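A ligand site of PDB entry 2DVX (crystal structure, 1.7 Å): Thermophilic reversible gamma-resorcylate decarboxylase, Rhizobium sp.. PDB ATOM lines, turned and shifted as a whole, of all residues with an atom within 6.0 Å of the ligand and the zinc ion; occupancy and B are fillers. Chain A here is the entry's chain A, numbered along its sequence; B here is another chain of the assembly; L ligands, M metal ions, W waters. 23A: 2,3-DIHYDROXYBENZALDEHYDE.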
ATOM      1  N   GLU A   8     -13.453   5.444  -2.674  1.00  0.00           N
ATOM      2  CA  GLU A   8     -12.578   5.855  -3.763  1.00  0.00           C
ATOM      3  C   GLU A   8     -11.238   5.323  -3.266  1.00  0.00           C
ATOM      4  O   GLU A   8     -10.360   6.063  -2.849  1.00  0.00           O
ATOM      5  CB  GLU A   8     -12.501   7.366  -3.995  1.00  0.00           C
ATOM      6  CG  GLU A   8     -11.712   7.632  -5.301  1.00  0.00           C
ATOM      7  CD  GLU A   8     -11.592   9.086  -5.718  1.00  0.00           C
ATOM      8  OE1 GLU A   8     -10.556   9.421  -6.329  1.00  0.00           O
ATOM      9  OE2 GLU A   8     -12.507   9.894  -5.465  1.00  0.00           O
ATOM     10  N   HIS A  10      -8.344   2.692  -4.463  1.00  0.00           N
ATOM     11  CA  HIS A  10      -7.809   2.031  -5.644  1.00  0.00           C
ATOM     12  C   HIS A  10      -6.806   0.906  -5.460  1.00  0.00           C
ATOM     13  O   HIS A  10      -6.184   0.748  -4.412  1.00  0.00           O
ATOM     14  CB  HIS A  10      -7.184   3.086  -6.548  1.00  0.00           C
ATOM     15  CG  HIS A  10      -8.067   4.276  -6.791  1.00  0.00           C
ATOM     16  ND1 HIS A  10      -9.212   4.210  -7.545  1.00  0.00           N
ATOM     17  CD2 HIS A  10      -7.961   5.559  -6.363  1.00  0.00           C
ATOM     18  CE1 HIS A  10      -9.782   5.402  -7.587  1.00  0.00           C
ATOM     19  NE2 HIS A  10      -9.044   6.243  -6.877  1.00  0.00           N
ATOM     20  N   ASP A  19       0.453   3.035 -15.187  1.00  0.00           N
ATOM     21  CA  ASP A  19      -0.383   4.211 -15.339  1.00  0.00           C
ATOM     22  C   ASP A  19      -0.228   5.159 -14.146  1.00  0.00           C
ATOM     23  O   ASP A  19      -0.438   6.372 -14.278  1.00  0.00           O
ATOM     24  CB  ASP A  19      -1.860   3.804 -15.452  1.00  0.00           C
ATOM     25  CG  ASP A  19      -2.259   3.466 -16.873  1.00  0.00           C
ATOM     26  OD1 ASP A  19      -1.385   3.064 -17.676  1.00  0.00           O
ATOM     27  OD2 ASP A  19      -3.457   3.598 -17.192  1.00  0.00           O
ATOM     28  N   SER A  20       0.143   4.611 -12.991  1.00  0.00           N
ATOM     29  CA  SER A  20       0.313   5.403 -11.778  1.00  0.00           C
ATOM     30  C   SER A  20       1.739   5.863 -11.503  1.00  0.00           C
ATOM     31  O   SER A  20       1.975   6.637 -10.572  1.00  0.00           O
ATOM     32  CB  SER A  20      -0.196   4.603 -10.568  1.00  0.00           C
ATOM     33  OG  SER A  20      -1.557   4.255 -10.717  1.00  0.00           O
ATOM     34  N   PHE A  23       2.788   9.812 -11.164  1.00  0.00           N
ATOM     35  CA  PHE A  23       2.124  10.696 -10.210  1.00  0.00           C
ATOM     36  C   PHE A  23       2.749  10.719  -8.822  1.00  0.00           C
ATOM     37  O   PHE A  23       2.139  11.200  -7.861  1.00  0.00           O
ATOM     38  CB  PHE A  23       0.641  10.345 -10.114  1.00  0.00           C
ATOM     39  CG  PHE A  23      -0.103  10.543 -11.415  1.00  0.00           C
ATOM     40  CD1 PHE A  23      -0.100   9.553 -12.392  1.00  0.00           C
ATOM     41  CD2 PHE A  23      -0.804  11.717 -11.649  1.00  0.00           C
ATOM     42  CE1 PHE A  23      -0.781   9.729 -13.589  1.00  0.00           C
ATOM     43  CE2 PHE A  23      -1.504  11.905 -12.846  1.00  0.00           C
ATOM     44  CZ  PHE A  23      -1.494  10.908 -13.820  1.00  0.00           C
ATOM     45  N   VAL A  24       3.970  10.200  -8.720  1.00  0.00           N
ATOM     46  CA  VAL A  24       4.721  10.188  -7.466  1.00  0.00           C
ATOM     47  C   VAL A  24       6.208  10.187  -7.817  1.00  0.00           C
ATOM     48  O   VAL A  24       6.617   9.563  -8.804  1.00  0.00           O
ATOM     49  CB  VAL A  24       4.424   8.930  -6.613  1.00  0.00           C
ATOM     50  CG1 VAL A  24       2.973   8.967  -6.136  1.00  0.00           C
ATOM     51  CG2 VAL A  24       4.696   7.666  -7.413  1.00  0.00           C
ATOM     52  N   ALA A  61      -6.183   4.740 -12.373  1.00  0.00           N
ATOM     53  CA  ALA A  61      -6.452   5.561 -13.550  1.00  0.00           C
ATOM     54  C   ALA A  61      -5.215   5.956 -14.360  1.00  0.00           C
ATOM     55  O   ALA A  61      -4.108   6.036 -13.824  1.00  0.00           O
ATOM     56  CB  ALA A  61      -7.193   6.825 -13.116  1.00  0.00           C
ATOM     57  N   HIS A 164     -14.724   9.391 -12.121  1.00  0.00           N
ATOM     58  CA  HIS A 164     -13.394   9.677 -11.574  1.00  0.00           C
ATOM     59  C   HIS A 164     -12.551  10.498 -12.553  1.00  0.00           C
ATOM     60  O   HIS A 164     -12.812  10.514 -13.747  1.00  0.00           O
ATOM     61  CB  HIS A 164     -12.717   8.327 -11.246  1.00  0.00           C
ATOM     62  CG  HIS A 164     -11.428   8.439 -10.489  1.00  0.00           C
ATOM     63  ND1 HIS A 164     -10.222   8.658 -11.108  1.00  0.00           N
ATOM     64  CD2 HIS A 164     -11.172   8.349  -9.159  1.00  0.00           C
ATOM     65  CE1 HIS A 164      -9.270   8.708 -10.190  1.00  0.00           C
ATOM     66  NE2 HIS A 164      -9.816   8.520  -9.002  1.00  0.00           N
ATOM     67  N   PRO A 165     -11.523  11.208 -12.046  1.00  0.00           N
ATOM     68  CA  PRO A 165     -10.670  12.016 -12.928  1.00  0.00           C
ATOM     69  C   PRO A 165      -9.676  11.275 -13.811  1.00  0.00           C
ATOM     70  O   PRO A 165      -9.410  10.083 -13.643  1.00  0.00           O
ATOM     71  CB  PRO A 165      -9.915  12.918 -11.953  1.00  0.00           C
ATOM     72  CG  PRO A 165     -10.783  12.959 -10.728  1.00  0.00           C
ATOM     73  CD  PRO A 165     -11.275  11.544 -10.637  1.00  0.00           C
ATOM     74  N   GLY A 184      -2.939  16.542 -13.166  1.00  0.00           N
ATOM     75  CA  GLY A 184      -3.214  15.626 -12.064  1.00  0.00           C
ATOM     76  C   GLY A 184      -4.082  16.196 -10.955  1.00  0.00           C
ATOM     77  O   GLY A 184      -4.878  17.113 -11.170  1.00  0.00           O
ATOM     78  N   PRO A 185      -3.931  15.677  -9.723  1.00  0.00           N
ATOM     79  CA  PRO A 185      -4.709  16.109  -8.567  1.00  0.00           C
ATOM     80  C   PRO A 185      -4.571  17.569  -8.133  1.00  0.00           C
ATOM     81  O   PRO A 185      -5.437  18.076  -7.406  1.00  0.00           O
ATOM     82  CB  PRO A 185      -4.263  15.130  -7.467  1.00  0.00           C
ATOM     83  CG  PRO A 185      -2.850  14.855  -7.842  1.00  0.00           C
ATOM     84  CD  PRO A 185      -2.932  14.651  -9.329  1.00  0.00           C
ATOM     85  N   PHE A 189      -7.194  17.450 -12.903  1.00  0.00           N
ATOM     86  CA  PHE A 189      -8.166  16.399 -12.610  1.00  0.00           C
ATOM     87  C   PHE A 189      -9.556  16.978 -12.315  1.00  0.00           C
ATOM     88  O   PHE A 189     -10.565  16.474 -12.820  1.00  0.00           O
ATOM     89  CB  PHE A 189      -7.738  15.593 -11.378  1.00  0.00           C
ATOM     90  CG  PHE A 189      -6.822  14.438 -11.675  1.00  0.00           C
ATOM     91  CD1 PHE A 189      -6.437  13.583 -10.643  1.00  0.00           C
ATOM     92  CD2 PHE A 189      -6.351  14.193 -12.961  1.00  0.00           C
ATOM     93  CE1 PHE A 189      -5.595  12.488 -10.893  1.00  0.00           C
ATOM     94  CE2 PHE A 189      -5.514  13.105 -13.214  1.00  0.00           C
ATOM     95  CZ  PHE A 189      -5.130  12.250 -12.182  1.00  0.00           C
ATOM     96  N   HIS A 218     -13.266  14.110  -4.469  1.00  0.00           N
ATOM     97  CA  HIS A 218     -12.601  15.386  -4.227  1.00  0.00           C
ATOM     98  C   HIS A 218     -13.561  16.530  -3.967  1.00  0.00           C
ATOM     99  O   HIS A 218     -13.364  17.654  -4.431  1.00  0.00           O
ATOM    100  CB  HIS A 218     -11.690  15.670  -5.412  1.00  0.00           C
ATOM    101  CG  HIS A 218     -11.013  14.429  -5.921  1.00  0.00           C
ATOM    102  ND1 HIS A 218     -11.433  13.764  -7.058  1.00  0.00           N
ATOM    103  CD2 HIS A 218     -10.058  13.644  -5.353  1.00  0.00           C
ATOM    104  CE1 HIS A 218     -10.770  12.624  -7.169  1.00  0.00           C
ATOM    105  NE2 HIS A 218      -9.935  12.526  -6.142  1.00  0.00           N
ATOM    106  N   SER A 262     -12.773  12.272  -0.800  1.00  0.00           N
ATOM    107  CA  SER A 262     -11.484  11.799  -1.273  1.00  0.00           C
ATOM    108  C   SER A 262     -10.495  12.908  -1.586  1.00  0.00           C
ATOM    109  O   SER A 262     -10.811  13.873  -2.280  1.00  0.00           O
ATOM    110  CB  SER A 262     -11.664  10.917  -2.514  1.00  0.00           C
ATOM    111  OG  SER A 262     -12.169  11.661  -3.609  1.00  0.00           O
ATOM    112  N   ASP A 287      -9.092   8.003  -1.124  1.00  0.00           N
ATOM    113  CA  ASP A 287      -8.284   8.050  -2.352  1.00  0.00           C
ATOM    114  C   ASP A 287      -6.990   7.276  -2.110  1.00  0.00           C
ATOM    115  O   ASP A 287      -5.957   7.533  -2.736  1.00  0.00           O
ATOM    116  CB  ASP A 287      -7.964   9.489  -2.786  1.00  0.00           C
ATOM    117  CG  ASP A 287      -7.967   9.644  -4.303  1.00  0.00           C
ATOM    118  OD1 ASP A 287      -7.995   8.604  -4.999  1.00  0.00           O
ATOM    119  OD2 ASP A 287      -7.950  10.803  -4.798  1.00  0.00           O
ATOM    120  N   PHE A 290      -3.163   6.821  -2.960  1.00  0.00           N
ATOM    121  CA  PHE A 290      -2.609   8.122  -3.327  1.00  0.00           C
ATOM    122  C   PHE A 290      -2.659   9.091  -2.150  1.00  0.00           C
ATOM    123  O   PHE A 290      -1.946  10.099  -2.119  1.00  0.00           O
ATOM    124  CB  PHE A 290      -3.369   8.663  -4.540  1.00  0.00           C
ATOM    125  CG  PHE A 290      -3.310   7.739  -5.721  1.00  0.00           C
ATOM    126  CD1 PHE A 290      -2.156   7.632  -6.481  1.00  0.00           C
ATOM    127  CD2 PHE A 290      -4.403   6.931  -6.046  1.00  0.00           C
ATOM    128  CE1 PHE A 290      -2.075   6.738  -7.552  1.00  0.00           C
ATOM    129  CE2 PHE A 290      -4.329   6.034  -7.111  1.00  0.00           C
ATOM    130  CZ  PHE A 290      -3.171   5.934  -7.864  1.00  0.00           C
ATOM    131  N   GLU A 291      -3.509   8.775  -1.184  1.00  0.00           N
ATOM    132  CA  GLU A 291      -3.645   9.545   0.057  1.00  0.00           C
ATOM    133  C   GLU A 291      -3.544   8.526   1.179  1.00  0.00           C
ATOM    134  O   GLU A 291      -3.978   7.391   1.024  1.00  0.00           O
ATOM    135  CB  GLU A 291      -5.025  10.213   0.153  1.00  0.00           C
ATOM    136  CG  GLU A 291      -5.321  11.241  -0.919  1.00  0.00           C
ATOM    137  CD  GLU A 291      -4.427  12.465  -0.843  1.00  0.00           C
ATOM    138  OE1 GLU A 291      -3.732  12.673   0.171  1.00  0.00           O
ATOM    139  OE2 GLU A 291      -4.439  13.245  -1.819  1.00  0.00           O
ATOM    140  N   ARG B 229      -6.549  21.424  -1.348  1.00  0.00           N
ATOM    141  CA  ARG B 229      -6.176  20.316  -2.210  1.00  0.00           C
ATOM    142  C   ARG B 229      -5.038  20.667  -3.174  1.00  0.00           C
ATOM    143  O   ARG B 229      -4.174  19.832  -3.430  1.00  0.00           O
ATOM    144  CB  ARG B 229      -7.406  19.831  -2.992  1.00  0.00           C
ATOM    145  CG  ARG B 229      -7.145  18.625  -3.903  1.00  0.00           C
ATOM    146  CD  ARG B 229      -8.454  17.979  -4.358  1.00  0.00           C
ATOM    147  NE  ARG B 229      -8.286  17.122  -5.520  1.00  0.00           N
ATOM    148  CZ  ARG B 229      -7.689  15.929  -5.523  1.00  0.00           C
ATOM    149  NH1 ARG B 229      -7.184  15.427  -4.404  1.00  0.00           N
ATOM    150  NH2 ARG B 229      -7.602  15.235  -6.639  1.00  0.00           N
ATOM    151  N   ASN B 234      -1.992  14.290  -2.009  1.00  0.00           N
ATOM    152  CA  ASN B 234      -0.894  13.331  -1.832  1.00  0.00           C
ATOM    153  C   ASN B 234       0.095  13.806  -0.770  1.00  0.00           C
ATOM    154  O   ASN B 234       1.307  13.745  -0.969  1.00  0.00           O
ATOM    155  CB  ASN B 234      -0.132  13.136  -3.148  1.00  0.00           C
ATOM    156  CG  ASN B 234      -1.050  12.892  -4.324  1.00  0.00           C
ATOM    157  OD1 ASN B 234      -1.958  12.079  -4.257  1.00  0.00           O
ATOM    158  ND2 ASN B 234      -0.784  13.600  -5.418  1.00  0.00           N
HETATM  159  C7  23A L   1      -6.442   9.469  -7.554  1.00  0.00           C
HETATM  160  O8  23A L   1      -7.304   8.651  -7.936  1.00  0.00           O
HETATM  161  C1  23A L   1      -5.234   9.581  -8.285  1.00  0.00           C
HETATM  162  C6  23A L   1      -5.072   8.743  -9.430  1.00  0.00           C
HETATM  163  C5  23A L   1      -3.877   8.792 -10.212  1.00  0.00           C
HETATM  164  C2  23A L   1      -4.206  10.473  -7.909  1.00  0.00           C
HETATM  165  O2  23A L   1      -4.290  11.314  -6.830  1.00  0.00           O
HETATM  166  C3  23A L   1      -3.004  10.524  -8.698  1.00  0.00           C
HETATM  167  C4  23A L   1      -2.865   9.692  -9.820  1.00  0.00           C
HETATM  168  O3  23A L   1      -2.019  11.356  -8.375  1.00  0.00           O
HETATM  169 ZN    ZN M   1      -8.957   8.385  -7.057  1.00  0.00          ZN
HETATM  170  O   HOH W   1      -6.858   6.052  -9.575  1.00  0.00           O
HETATM  171  O   HOH W   2      -6.840  12.571  -7.163  1.00  0.00           O
HETATM  172  O   HOH W   3      -3.304   5.965 -11.298  1.00  0.00           O
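Four residues have an atom within 4 Å of the zinc ion: Glu 8, His 10, His 164 and Asp 287.
The backbone NH (N) of Phe 189 sits at hydrogen-bond distance from the backbone carbonyl oxygen (O) of Gly 184 (2.9 Å). O of Phe 290 lies close to OD1 of Asn 234 of chain B (2.9 Å). OD2 of Asp 287 sits at hydrogen-bond distance from NE2 of His 218, at 3.0 Å. The side-chain carboxylate (OE2) of Glu 8 sits at hydrogen-bond distance from the side-chain hydroxyl (OG) of Ser 262. OE2 of Glu 291 lies within hydrogen-bond range of N of Asn 234 of chain B. OE1 of Glu 8 lies close to NE2 of His 218 (3.2 Å).
Water W2 lies within hydrogen-bond range of the guanidinium group of Arg 229 of chain B (2.8 Å), an oxygen (O2) of the ligand (2.9 Å), the side-chain carboxylate of Asp 287 (3.2 Å) and a ring nitrogen (NE2) of His 218 (3.3 Å). Water W3 bridges OG of Ser 20 (2.5 Å) and O of Ala 61 (2.7 Å).
CG of Phe 23 touches C4 of the ligand, at 3.3 Å. Pro 185 touches the ligand (CD to O3, 3.5 Å). CE1 of Phe 189 touches C2 of the ligand (3.9 Å). Phe 290 touches the ligand (CD2 to C1, 3.6 Å). Asn 234 of chain B touches the ligand. Hydrophobic or aromatic side chains that line the ligand: His 10, Phe 23, His 164, Pro 185, Phe 189 and Phe 290. Within 4 Å of the ligand: Glu 8, His 10, Phe 23, His 164, Pro 185, Phe 189, Asp 287, Phe 290 and Asn 234 of chain B. Along chain A the residues within 4 Å of the ligand span positions 8 to 290. The nearest printed residue that does not touch the ligand is Ala 61 (4.5 Å).
O8 of the ligand is bound to the zinc ion, at 1.9 Å. The side-chain carboxylate (OE1) of Glu 8 binds the zinc ion (2.0 Å). The zinc ion is bound by a ring nitrogen (NE2) of His 164 (2.1 Å). NE2 of His 10 is bound to the zinc ion (2.2 Å). OD1 of Asp 287 is bound to the zinc ion (2.3 Å).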
